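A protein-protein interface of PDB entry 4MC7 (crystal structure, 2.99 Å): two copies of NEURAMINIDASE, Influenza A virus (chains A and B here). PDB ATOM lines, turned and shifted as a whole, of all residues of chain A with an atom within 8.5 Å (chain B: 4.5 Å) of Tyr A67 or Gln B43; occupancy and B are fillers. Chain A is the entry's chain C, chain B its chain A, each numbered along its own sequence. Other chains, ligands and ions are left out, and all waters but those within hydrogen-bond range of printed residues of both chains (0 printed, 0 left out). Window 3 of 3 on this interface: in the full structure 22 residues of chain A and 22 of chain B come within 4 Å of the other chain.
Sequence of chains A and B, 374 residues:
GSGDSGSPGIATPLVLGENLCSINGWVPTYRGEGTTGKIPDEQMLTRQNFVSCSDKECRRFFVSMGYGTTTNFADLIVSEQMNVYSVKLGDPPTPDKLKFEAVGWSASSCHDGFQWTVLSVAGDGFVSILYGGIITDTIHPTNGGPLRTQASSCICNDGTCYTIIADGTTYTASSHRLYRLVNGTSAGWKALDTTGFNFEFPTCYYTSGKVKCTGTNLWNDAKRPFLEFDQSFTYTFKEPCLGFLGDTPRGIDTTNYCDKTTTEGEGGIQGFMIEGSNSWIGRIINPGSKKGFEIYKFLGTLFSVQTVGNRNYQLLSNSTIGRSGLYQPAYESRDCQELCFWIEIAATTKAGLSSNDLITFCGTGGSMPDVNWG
Tyr A67 touches Pro B40, but with the chains exchanged Pro A40 does not touch Tyr B67 (19.1 Å).
Tyr A67 touches Gln B43, but with the chains exchanged Gln A43 does not touch Tyr B67 (17.0 Å).
Positions printed for both chains: 40, 41, 42, 43, 44, 45, 67, 68, 93 and 94.
Of chain B, only Glu B33 (3.5 Å), Pro B40 (3.5 Å) and Gln B43 (3.9 Å) come within 4 Å of Tyr A67.
Of chain A, only Tyr A67 comes within 4 Å of Gln B43.
No residue of chain A comes within 4 Å of Pro B93.
Of the printed residues of chain B, Thr A70 touches Pro B40 (3.8 Å).
Of the printed residues of chain B, Pro A95 touches Pro B92 (3.6 Å).
Printed residues of chain A within 4 Å of Glu B33: Met A44, Ser A64, Tyr A67 and Tyr A85.
The backbone carbonyl oxygen (O) of Tyr A67 lies within hydrogen-bond range of the side-chain hydroxyl (OG1) of Thr A70, at 3.4 Å.
The backbone carbonyl oxygen of Pro A93 lies within hydrogen-bond range of the backbone NH of Met A44, at 3.0 Å.
OG1 of Thr A71 lies within hydrogen-bond range of O of Tyr A67.
O of Gln B43 sits at hydrogen-bond distance from N of Gly B68, at 3.1 Å.
Glu B33 touches Met A44.
OE2 of Glu B33 touches OG of Ser A64 (3.6 Å).
CG of Glu B33 touches CE2 of Tyr A67, at 3.5 Å.
CG of Pro B40 touches CD2 of Tyr A67 (3.5 Å).
NE2 of Gln B43 touches OH of Tyr A67, 3.9 Å away.
Thr A70 touches Pro B40 (CG2 to N, 3.8 Å).
CG of Pro B92 touches O of Pro A95 (3.6 Å).
The side-chain hydroxyl (OG1) of Thr B94 lies within hydrogen-bond range of the side-chain carboxylate (OD1) of Asp A96, 3.0 Å away.
The side-chain hydroxyl of Tyr A85 sits close to the side-chain carboxylate of Glu B33 (2.2 Å).
Of the 25 printed residues of chain A, 7 touch a printed residue of chain B.
Printed residues of chain A that touch a printed residue of chain B: Met A44, Ser A64, Tyr A67, Thr A70, Tyr A85, Pro A95 and Asp A96.
Hydrophobic or aromatic side chains of chain A within 4 Å of the printed part of chain B: Met A44, Tyr A67 and Tyr A85.
Along chain A the printed residues that touch a printed residue of chain B span positions 44 to 96.
Of the 13 printed residues of chain B, 5 touch a printed residue of chain A.
Hydrophobic or aromatic side chains of chain B that line the printed part of chain A: Pro B40 and Pro B92.
Among the printed residues, 9 pairs touch across the chains.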
ATOM      1  N   PRO A  40      13.147  20.419  16.494  1.00  0.00           N
ATOM      2  CA  PRO A  40      12.641  19.383  15.570  1.00  0.00           C
ATOM      3  C   PRO A  40      13.755  18.686  14.791  1.00  0.00           C
ATOM      4  O   PRO A  40      14.686  19.351  14.297  1.00  0.00           O
ATOM      5  CB  PRO A  40      11.774  20.181  14.598  1.00  0.00           C
ATOM      6  CG  PRO A  40      11.414  21.439  15.330  1.00  0.00           C
ATOM      7  CD  PRO A  40      12.576  21.749  16.205  1.00  0.00           C
ATOM      8  N   ASP A  41      13.654  17.362  14.669  1.00  0.00           N
ATOM      9  CA  ASP A  41      14.762  16.554  14.138  1.00  0.00           C
ATOM     10  C   ASP A  41      15.091  16.862  12.689  1.00  0.00           C
ATOM     11  O   ASP A  41      16.221  16.634  12.252  1.00  0.00           O
ATOM     12  CB  ASP A  41      14.511  15.057  14.325  1.00  0.00           C
ATOM     13  CG  ASP A  41      14.244  14.689  15.774  1.00  0.00           C
ATOM     14  OD1 ASP A  41      13.820  15.575  16.535  1.00  0.00           O
ATOM     15  OD2 ASP A  41      14.446  13.519  16.155  1.00  0.00           O
ATOM     16  N   GLU A  42      14.114  17.392  11.954  1.00  0.00           N
ATOM     17  CA  GLU A  42      14.311  17.709  10.541  1.00  0.00           C
ATOM     18  C   GLU A  42      15.143  18.952  10.308  1.00  0.00           C
ATOM     19  O   GLU A  42      15.667  19.143   9.207  1.00  0.00           O
ATOM     20  CB  GLU A  42      13.001  17.817   9.769  1.00  0.00           C
ATOM     21  CG  GLU A  42      12.108  18.979  10.139  1.00  0.00           C
ATOM     22  CD  GLU A  42      10.902  18.537  10.964  1.00  0.00           C
ATOM     23  OE1 GLU A  42      11.080  17.788  11.953  1.00  0.00           O
ATOM     24  OE2 GLU A  42       9.768  18.938  10.620  1.00  0.00           O
ATOM     25  N   GLN A  43      15.277  19.793  11.329  1.00  0.00           N
ATOM     26  CA  GLN A  43      16.119  20.977  11.190  1.00  0.00           C
ATOM     27  C   GLN A  43      17.595  20.630  11.030  1.00  0.00           C
ATOM     28  O   GLN A  43      18.059  19.567  11.451  1.00  0.00           O
ATOM     29  CB  GLN A  43      15.920  21.920  12.359  1.00  0.00           C
ATOM     30  CG  GLN A  43      14.586  22.625  12.337  1.00  0.00           C
ATOM     31  CD  GLN A  43      14.570  23.854  13.208  1.00  0.00           C
ATOM     32  OE1 GLN A  43      15.611  24.464  13.463  1.00  0.00           O
ATOM     33  NE2 GLN A  43      13.386  24.234  13.668  1.00  0.00           N
ATOM     34  N   MET A  44      18.314  21.520  10.367  1.00  0.00           N
ATOM     35  CA  MET A  44      19.755  21.428  10.231  1.00  0.00           C
ATOM     36  C   MET A  44      20.370  21.745  11.621  1.00  0.00           C
ATOM     37  O   MET A  44      19.905  22.632  12.344  1.00  0.00           O
ATOM     38  CB  MET A  44      20.200  22.423   9.158  1.00  0.00           C
ATOM     39  CG  MET A  44      21.678  22.441   8.892  1.00  0.00           C
ATOM     40  SD  MET A  44      22.201  20.948   8.049  1.00  0.00           S
ATOM     41  CE  MET A  44      21.958  21.375   6.317  1.00  0.00           C
ATOM     42  N   LEU A  45      21.373  20.974  12.022  1.00  0.00           N
ATOM     43  CA  LEU A  45      22.112  21.255  13.255  1.00  0.00           C
ATOM     44  C   LEU A  45      23.102  22.371  12.961  1.00  0.00           C
ATOM     45  O   LEU A  45      23.827  22.309  11.969  1.00  0.00           O
ATOM     46  CB  LEU A  45      22.883  20.013  13.716  1.00  0.00           C
ATOM     47  CG  LEU A  45      22.103  18.725  13.991  1.00  0.00           C
ATOM     48  CD1 LEU A  45      23.094  17.581  14.139  1.00  0.00           C
ATOM     49  CD2 LEU A  45      21.221  18.862  15.228  1.00  0.00           C
ATOM     50  N   THR A  46      23.147  23.394  13.802  1.00  0.00           N
ATOM     51  CA  THR A  46      23.994  24.550  13.495  1.00  0.00           C
ATOM     52  C   THR A  46      25.077  24.749  14.510  1.00  0.00           C
ATOM     53  O   THR A  46      24.960  24.361  15.677  1.00  0.00           O
ATOM     54  CB  THR A  46      23.216  25.880  13.457  1.00  0.00           C
ATOM     55  OG1 THR A  46      22.755  26.192  14.768  1.00  0.00           O
ATOM     56  CG2 THR A  46      22.026  25.808  12.539  1.00  0.00           C
ATOM     57  N   SER A  64      26.864  24.058   9.188  1.00  0.00           N
ATOM     58  CA  SER A  64      26.042  22.860   9.346  1.00  0.00           C
ATOM     59  C   SER A  64      26.805  21.711   9.970  1.00  0.00           C
ATOM     60  O   SER A  64      27.998  21.512   9.701  1.00  0.00           O
ATOM     61  CB  SER A  64      25.499  22.391   8.002  1.00  0.00           C
ATOM     62  OG  SER A  64      26.545  21.886   7.193  1.00  0.00           O
ATOM     63  N   MET A  65      26.103  20.957  10.802  1.00  0.00           N
ATOM     64  CA  MET A  65      26.592  19.667  11.257  1.00  0.00           C
ATOM     65  C   MET A  65      25.817  18.501  10.601  1.00  0.00           C
ATOM     66  O   MET A  65      26.050  17.327  10.918  1.00  0.00           O
ATOM     67  CB  MET A  65      26.556  19.561  12.789  1.00  0.00           C
ATOM     68  CG  MET A  65      27.846  19.968  13.493  1.00  0.00           C
ATOM     69  SD  MET A  65      27.665  21.368  14.625  1.00  0.00           S
ATOM     70  CE  MET A  65      26.951  20.579  16.084  1.00  0.00           C
ATOM     71  N   GLY A  66      24.924  18.815   9.665  1.00  0.00           N
ATOM     72  CA  GLY A  66      24.056  17.786   9.097  1.00  0.00           C
ATOM     73  C   GLY A  66      22.660  17.910   9.683  1.00  0.00           C
ATOM     74  O   GLY A  66      22.431  18.693  10.604  1.00  0.00           O
ATOM     75  N   TYR A  67      21.712  17.164   9.135  1.00  0.00           N
ATOM     76  CA  TYR A  67      20.354  17.205   9.646  1.00  0.00           C
ATOM     77  C   TYR A  67      20.270  16.374  10.912  1.00  0.00           C
ATOM     78  O   TYR A  67      20.989  15.386  11.063  1.00  0.00           O
ATOM     79  CB  TYR A  67      19.394  16.652   8.617  1.00  0.00           C
ATOM     80  CG  TYR A  67      19.418  17.386   7.304  1.00  0.00           C
ATOM     81  CD1 TYR A  67      18.884  18.668   7.187  1.00  0.00           C
ATOM     82  CD2 TYR A  67      19.954  16.793   6.168  1.00  0.00           C
ATOM     83  CE1 TYR A  67      18.891  19.340   5.963  1.00  0.00           C
ATOM     84  CE2 TYR A  67      19.954  17.450   4.944  1.00  0.00           C
ATOM     85  CZ  TYR A  67      19.426  18.721   4.852  1.00  0.00           C
ATOM     86  OH  TYR A  67      19.430  19.358   3.635  1.00  0.00           O
ATOM     87  N   GLY A  68      19.391  16.774  11.822  1.00  0.00           N
ATOM     88  CA  GLY A  68      19.258  16.093  13.110  1.00  0.00           C
ATOM     89  C   GLY A  68      18.683  14.687  13.027  1.00  0.00           C
ATOM     90  O   GLY A  68      18.892  13.865  13.918  1.00  0.00           O
ATOM     91  N   THR A  69      17.956  14.417  11.954  1.00  0.00           N
ATOM     92  CA  THR A  69      17.342  13.120  11.748  1.00  0.00           C
ATOM     93  C   THR A  69      18.293  12.099  11.103  1.00  0.00           C
ATOM     94  O   THR A  69      18.193  10.886  11.353  1.00  0.00           O
ATOM     95  CB  THR A  69      16.016  13.242  10.938  1.00  0.00           C
ATOM     96  OG1 THR A  69      15.514  11.936  10.646  1.00  0.00           O
ATOM     97  CG2 THR A  69      16.186  14.013   9.628  1.00  0.00           C
ATOM     98  N   THR A  70      19.214  12.599  10.286  1.00  0.00           N
ATOM     99  CA  THR A  70      20.133  11.749   9.543  1.00  0.00           C
ATOM    100  C   THR A  70      21.431  11.570  10.318  1.00  0.00           C
ATOM    101  O   THR A  70      22.304  10.800   9.898  1.00  0.00           O
ATOM    102  CB  THR A  70      20.445  12.343   8.155  1.00  0.00           C
ATOM    103  OG1 THR A  70      21.404  13.406   8.277  1.00  0.00           O
ATOM    104  CG2 THR A  70      19.175  12.876   7.507  1.00  0.00           C
ATOM    105  N   THR A  71      21.545  12.287  11.441  1.00  0.00           N
ATOM    106  CA  THR A  71      22.742  12.254  12.275  1.00  0.00           C
ATOM    107  C   THR A  71      22.506  11.371  13.490  1.00  0.00           C
ATOM    108  O   THR A  71      21.543  11.575  14.218  1.00  0.00           O
ATOM    109  CB  THR A  71      23.156  13.679  12.744  1.00  0.00           C
ATOM    110  OG1 THR A  71      23.536  14.475  11.612  1.00  0.00           O
ATOM    111  CG2 THR A  71      24.321  13.622  13.745  1.00  0.00           C
ATOM    112  N   ASN A  72      23.386  10.392  13.697  1.00  0.00           N
ATOM    113  CA  ASN A  72      23.334   9.541  14.885  1.00  0.00           C
ATOM    114  C   ASN A  72      24.284  10.072  15.962  1.00  0.00           C
ATOM    115  O   ASN A  72      25.346  10.606  15.640  1.00  0.00           O
ATOM    116  CB  ASN A  72      23.640   8.074  14.533  1.00  0.00           C
ATOM    117  CG  ASN A  72      23.216   7.111  15.625  1.00  0.00           C
ATOM    118  OD1 ASN A  72      22.368   7.431  16.461  1.00  0.00           O
ATOM    119  ND2 ASN A  72      23.807   5.924  15.625  1.00  0.00           N
ATOM    120  N   ILE A  77      31.076  14.418  14.417  1.00  0.00           N
ATOM    121  CA  ILE A  77      31.265  14.944  13.068  1.00  0.00           C
ATOM    122  C   ILE A  77      32.438  15.931  12.985  1.00  0.00           C
ATOM    123  O   ILE A  77      32.842  16.557  13.974  1.00  0.00           O
ATOM    124  CB  ILE A  77      29.972  15.548  12.469  1.00  0.00           C
ATOM    125  CG1 ILE A  77      30.123  15.692  10.943  1.00  0.00           C
ATOM    126  CG2 ILE A  77      29.628  16.881  13.161  1.00  0.00           C
ATOM    127  CD1 ILE A  77      28.843  15.519  10.132  1.00  0.00           C
ATOM    128  N   TYR A  85      25.990  27.720   5.693  1.00  0.00           N
ATOM    129  CA  TYR A  85      24.636  28.137   5.298  1.00  0.00           C
ATOM    130  C   TYR A  85      24.218  29.500   5.797  1.00  0.00           C
ATOM    131  O   TYR A  85      24.749  30.037   6.782  1.00  0.00           O
ATOM    132  CB  TYR A  85      23.622  27.119   5.764  1.00  0.00           C
ATOM    133  CG  TYR A  85      23.728  25.823   4.999  1.00  0.00           C
ATOM    134  CD1 TYR A  85      23.150  25.676   3.731  1.00  0.00           C
ATOM    135  CD2 TYR A  85      24.412  24.743   5.534  1.00  0.00           C
ATOM    136  CE1 TYR A  85      23.251  24.502   3.036  1.00  0.00           C
ATOM    137  CE2 TYR A  85      24.506  23.547   4.846  1.00  0.00           C
ATOM    138  CZ  TYR A  85      23.930  23.432   3.596  1.00  0.00           C
ATOM    139  OH  TYR A  85      24.049  22.246   2.907  1.00  0.00           O
ATOM    140  N   PRO A  93      16.144  27.087  10.681  1.00  0.00           N
ATOM    141  CA  PRO A  93      16.952  26.393   9.687  1.00  0.00           C
ATOM    142  C   PRO A  93      16.335  25.091   9.221  1.00  0.00           C
ATOM    143  O   PRO A  93      16.890  24.030   9.446  1.00  0.00           O
ATOM    144  CB  PRO A  93      18.283  26.156  10.416  1.00  0.00           C
ATOM    145  CG  PRO A  93      17.945  26.243  11.845  1.00  0.00           C
ATOM    146  CD  PRO A  93      16.859  27.241  11.958  1.00  0.00           C
ATOM    147  N   THR A  94      15.171  25.182   8.594  1.00  0.00           N
ATOM    148  CA  THR A  94      14.577  24.048   7.898  1.00  0.00           C
ATOM    149  C   THR A  94      15.267  23.947   6.558  1.00  0.00           C
ATOM    150  O   THR A  94      15.829  24.944   6.090  1.00  0.00           O
ATOM    151  CB  THR A  94      13.056  24.216   7.664  1.00  0.00           C
ATOM    152  OG1 THR A  94      12.770  25.539   7.190  1.00  0.00           O
ATOM    153  CG2 THR A  94      12.260  23.929   8.958  1.00  0.00           C
ATOM    154  N   PRO A  95      15.248  22.748   5.943  1.00  0.00           N
ATOM    155  CA  PRO A  95      15.893  22.468   4.646  1.00  0.00           C
ATOM    156  C   PRO A  95      15.424  23.388   3.537  1.00  0.00           C
ATOM    157  O   PRO A  95      16.216  23.778   2.670  1.00  0.00           O
ATOM    158  CB  PRO A  95      15.459  21.044   4.338  1.00  0.00           C
ATOM    159  CG  PRO A  95      15.274  20.431   5.683  1.00  0.00           C
ATOM    160  CD  PRO A  95      14.717  21.519   6.558  1.00  0.00           C
ATOM    161  N   ASP A  96      14.151  23.749   3.589  1.00  0.00           N
ATOM    162  CA  ASP A  96      13.574  24.657   2.611  1.00  0.00           C
ATOM    163  C   ASP A  96      13.983  26.122   2.783  1.00  0.00           C
ATOM    164  O   ASP A  96      13.961  26.872   1.818  1.00  0.00           O
ATOM    165  CB  ASP A  96      12.065  24.525   2.639  1.00  0.00           C
ATOM    166  CG  ASP A  96      11.622  23.086   2.669  1.00  0.00           C
ATOM    167  OD1 ASP A  96      12.408  22.223   2.244  1.00  0.00           O
ATOM    168  OD2 ASP A  96      10.493  22.810   3.121  1.00  0.00           O
ATOM    169  N   LEU A  98      17.046  27.041   3.996  1.00  0.00           N
ATOM    170  CA  LEU A  98      18.508  27.155   3.940  1.00  0.00           C
ATOM    171  C   LEU A  98      18.974  27.698   2.630  1.00  0.00           C
ATOM    172  O   LEU A  98      18.386  27.440   1.594  1.00  0.00           O
ATOM    173  CB  LEU A  98      19.180  25.811   4.162  1.00  0.00           C
ATOM    174  CG  LEU A  98      19.065  25.207   5.552  1.00  0.00           C
ATOM    175  CD1 LEU A  98      20.220  24.278   5.726  1.00  0.00           C
ATOM    176  CD2 LEU A  98      19.067  26.256   6.667  1.00  0.00           C
ATOM    177  N   THR A 349      18.213  18.565  20.129  1.00  0.00           N
ATOM    178  CA  THR A 349      17.194  18.064  19.222  1.00  0.00           C
ATOM    179  C   THR A 349      16.167  17.281  20.036  1.00  0.00           C
ATOM    180  O   THR A 349      16.400  16.963  21.207  1.00  0.00           O
ATOM    181  CB  THR A 349      17.869  17.212  18.143  1.00  0.00           C
ATOM    182  OG1 THR A 349      18.703  18.077  17.364  1.00  0.00           O
ATOM    183  CG2 THR A 349      16.880  16.500  17.227  1.00  0.00           C
ATOM    184  N   LEU A 353      21.620  15.364  20.883  1.00  0.00           N
ATOM    185  CA  LEU A 353      22.271  16.244  19.892  1.00  0.00           C
ATOM    186  C   LEU A 353      22.353  17.686  20.390  1.00  0.00           C
ATOM    187  O   LEU A 353      21.448  18.138  21.069  1.00  0.00           O
ATOM    188  CB  LEU A 353      21.579  16.147  18.523  1.00  0.00           C
ATOM    189  CG  LEU A 353      21.063  14.734  18.128  1.00  0.00           C
ATOM    190  CD1 LEU A 353      20.082  14.740  16.971  1.00  0.00           C
ATOM    191  CD2 LEU A 353      22.162  13.724  17.840  1.00  0.00           C
ATOM    192  N   GLU B  33      24.140  17.694   0.559  1.00  0.00           N
ATOM    193  CA  GLU B  33      24.212  17.249   1.934  1.00  0.00           C
ATOM    194  C   GLU B  33      24.375  15.739   2.017  1.00  0.00           C
ATOM    195  O   GLU B  33      24.814  15.218   3.038  1.00  0.00           O
ATOM    196  CB  GLU B  33      23.015  17.743   2.743  1.00  0.00           C
ATOM    197  CG  GLU B  33      23.370  18.037   4.218  1.00  0.00           C
ATOM    198  CD  GLU B  33      24.380  19.185   4.416  1.00  0.00           C
ATOM    199  OE1 GLU B  33      24.305  20.199   3.695  1.00  0.00           O
ATOM    200  OE2 GLU B  33      25.242  19.075   5.315  1.00  0.00           O
ATOM    201  N   ILE B  39      20.691  11.018   3.449  1.00  0.00           N
ATOM    202  CA  ILE B  39      19.646  11.867   2.892  1.00  0.00           C
ATOM    203  C   ILE B  39      18.346  11.685   3.655  1.00  0.00           C
ATOM    204  O   ILE B  39      17.950  10.550   3.948  1.00  0.00           O
ATOM    205  CB  ILE B  39      19.405  11.552   1.414  1.00  0.00           C
ATOM    206  CG1 ILE B  39      20.734  11.352   0.668  1.00  0.00           C
ATOM    207  CG2 ILE B  39      18.471  12.607   0.756  1.00  0.00           C
ATOM    208  CD1 ILE B  39      21.193  12.510  -0.158  1.00  0.00           C
ATOM    209  N   PRO B  40      17.676  12.804   3.986  1.00  0.00           N
ATOM    210  CA  PRO B  40      16.329  12.764   4.590  1.00  0.00           C
ATOM    211  C   PRO B  40      15.302  12.075   3.683  1.00  0.00           C
ATOM    212  O   PRO B  40      15.266  12.319   2.482  1.00  0.00           O
ATOM    213  CB  PRO B  40      15.974  14.244   4.757  1.00  0.00           C
ATOM    214  CG  PRO B  40      17.289  14.957   4.770  1.00  0.00           C
ATOM    215  CD  PRO B  40      18.225  14.172   3.909  1.00  0.00           C
ATOM    216  N   ASP B  41      14.456  11.242   4.264  1.00  0.00           N
ATOM    217  CA  ASP B  41      13.570  10.390   3.487  1.00  0.00           C
ATOM    218  C   ASP B  41      12.565  11.156   2.645  1.00  0.00           C
ATOM    219  O   ASP B  41      12.108  10.648   1.624  1.00  0.00           O
ATOM    220  CB  ASP B  41      12.862   9.383   4.401  1.00  0.00           C
ATOM    221  CG  ASP B  41      13.844   8.555   5.225  1.00  0.00           C
ATOM    222  OD1 ASP B  41      14.972   9.030   5.433  1.00  0.00           O
ATOM    223  OD2 ASP B  41      13.509   7.439   5.667  1.00  0.00           O
ATOM    224  N   GLU B  42      12.228  12.374   3.061  1.00  0.00           N
ATOM    225  CA  GLU B  42      11.224  13.157   2.336  1.00  0.00           C
ATOM    226  C   GLU B  42      11.750  13.735   1.019  1.00  0.00           C
ATOM    227  O   GLU B  42      10.957  14.152   0.167  1.00  0.00           O
ATOM    228  CB  GLU B  42      10.602  14.263   3.198  1.00  0.00           C
ATOM    229  CG  GLU B  42      11.558  15.375   3.593  1.00  0.00           C
ATOM    230  CD  GLU B  42      11.983  15.274   5.042  1.00  0.00           C
ATOM    231  OE1 GLU B  42      12.350  14.159   5.489  1.00  0.00           O
ATOM    232  OE2 GLU B  42      11.936  16.317   5.733  1.00  0.00           O
ATOM    233  N   GLN B  43      13.072  13.766   0.851  1.00  0.00           N
ATOM    234  CA  GLN B  43      13.646  14.242  -0.388  1.00  0.00           C
ATOM    235  C   GLN B  43      13.345  13.310  -1.555  1.00  0.00           C
ATOM    236  O   GLN B  43      13.163  12.106  -1.377  1.00  0.00           O
ATOM    237  CB  GLN B  43      15.137  14.447  -0.247  1.00  0.00           C
ATOM    238  CG  GLN B  43      15.504  15.691   0.542  1.00  0.00           C
ATOM    239  CD  GLN B  43      16.952  16.120   0.337  1.00  0.00           C
ATOM    240  OE1 GLN B  43      17.552  15.868  -0.727  1.00  0.00           O
ATOM    241  NE2 GLN B  43      17.527  16.772   1.362  1.00  0.00           N
ATOM    242  N   MET B  44      13.260  13.902  -2.746  1.00  0.00           N
ATOM    243  CA  MET B  44      13.141  13.177  -4.000  1.00  0.00           C
ATOM    244  C   MET B  44      14.446  12.426  -4.222  1.00  0.00           C
ATOM    245  O   MET B  44      15.502  13.001  -4.023  1.00  0.00           O
ATOM    246  CB  MET B  44      12.929  14.190  -5.119  1.00  0.00           C
ATOM    247  CG  MET B  44      12.733  13.577  -6.487  1.00  0.00           C
ATOM    248  SD  MET B  44      11.204  12.651  -6.585  1.00  0.00           S
ATOM    249  CE  MET B  44       9.990  13.889  -7.067  1.00  0.00           C
ATOM    250  N   LEU B  45      14.386  11.149  -4.587  1.00  0.00           N
ATOM    251  CA  LEU B  45      15.596  10.395  -4.962  1.00  0.00           C
ATOM    252  C   LEU B  45      16.003  10.847  -6.360  1.00  0.00           C
ATOM    253  O   LEU B  45      15.138  10.902  -7.246  1.00  0.00           O
ATOM    254  CB  LEU B  45      15.326   8.892  -5.009  1.00  0.00           C
ATOM    255  CG  LEU B  45      14.769   8.237  -3.750  1.00  0.00           C
ATOM    256  CD1 LEU B  45      14.288   6.832  -4.020  1.00  0.00           C
ATOM    257  CD2 LEU B  45      15.801   8.224  -2.689  1.00  0.00           C
ATOM    258  N   TYR B  67       9.870   9.683  -4.250  1.00  0.00           N
ATOM    259  CA  TYR B  67      10.275  10.152  -2.931  1.00  0.00           C
ATOM    260  C   TYR B  67      10.858   8.981  -2.175  1.00  0.00           C
ATOM    261  O   TYR B  67      10.447   7.846  -2.372  1.00  0.00           O
ATOM    262  CB  TYR B  67       9.081  10.743  -2.178  1.00  0.00           C
ATOM    263  CG  TYR B  67       8.418  11.912  -2.882  1.00  0.00           C
ATOM    264  CD1 TYR B  67       9.063  13.148  -2.998  1.00  0.00           C
ATOM    265  CD2 TYR B  67       7.148  11.783  -3.429  1.00  0.00           C
ATOM    266  CE1 TYR B  67       8.449  14.224  -3.649  1.00  0.00           C
ATOM    267  CE2 TYR B  67       6.526  12.847  -4.071  1.00  0.00           C
ATOM    268  CZ  TYR B  67       7.178  14.065  -4.182  1.00  0.00           C
ATOM    269  OH  TYR B  67       6.551  15.124  -4.819  1.00  0.00           O
ATOM    270  N   GLY B  68      11.814   9.262  -1.301  1.00  0.00           N
ATOM    271  CA  GLY B  68      12.474   8.222  -0.517  1.00  0.00           C
ATOM    272  C   GLY B  68      11.599   7.571   0.541  1.00  0.00           C
ATOM    273  O   GLY B  68      11.865   6.454   0.958  1.00  0.00           O
ATOM    274  N   PRO B  92      18.311  21.899  -1.914  1.00  0.00           N
ATOM    275  CA  PRO B  92      18.139  20.466  -1.853  1.00  0.00           C
ATOM    276  C   PRO B  92      16.855  20.084  -2.568  1.00  0.00           C
ATOM    277  O   PRO B  92      15.938  20.892  -2.600  1.00  0.00           O
ATOM    278  CB  PRO B  92      18.030  20.217  -0.355  1.00  0.00           C
ATOM    279  CG  PRO B  92      17.363  21.441   0.167  1.00  0.00           C
ATOM    280  CD  PRO B  92      17.982  22.549  -0.633  1.00  0.00           C
ATOM    281  N   PRO B  93      16.785  18.870  -3.145  1.00  0.00           N
ATOM    282  CA  PRO B  93      15.537  18.375  -3.781  1.00  0.00           C
ATOM    283  C   PRO B  93      14.390  17.998  -2.826  1.00  0.00           C
ATOM    284  O   PRO B  93      13.912  16.877  -2.843  1.00  0.00           O
ATOM    285  CB  PRO B  93      16.001  17.166  -4.616  1.00  0.00           C
ATOM    286  CG  PRO B  93      17.292  16.735  -3.952  1.00  0.00           C
ATOM    287  CD  PRO B  93      17.943  18.022  -3.478  1.00  0.00           C
ATOM    288  N   THR B  94      13.939  18.955  -2.022  1.00  0.00           N
ATOM    289  CA  THR B  94      12.671  18.830  -1.297  1.00  0.00           C
ATOM    290  C   THR B  94      11.515  19.060  -2.255  1.00  0.00           C
ATOM    291  O   THR B  94      11.634  19.798  -3.234  1.00  0.00           O
ATOM    292  CB  THR B  94      12.536  19.827  -0.117  1.00  0.00           C
ATOM    293  OG1 THR B  94      12.971  21.125  -0.532  1.00  0.00           O
ATOM    294  CG2 THR B  94      13.376  19.380   1.064  1.00  0.00           C
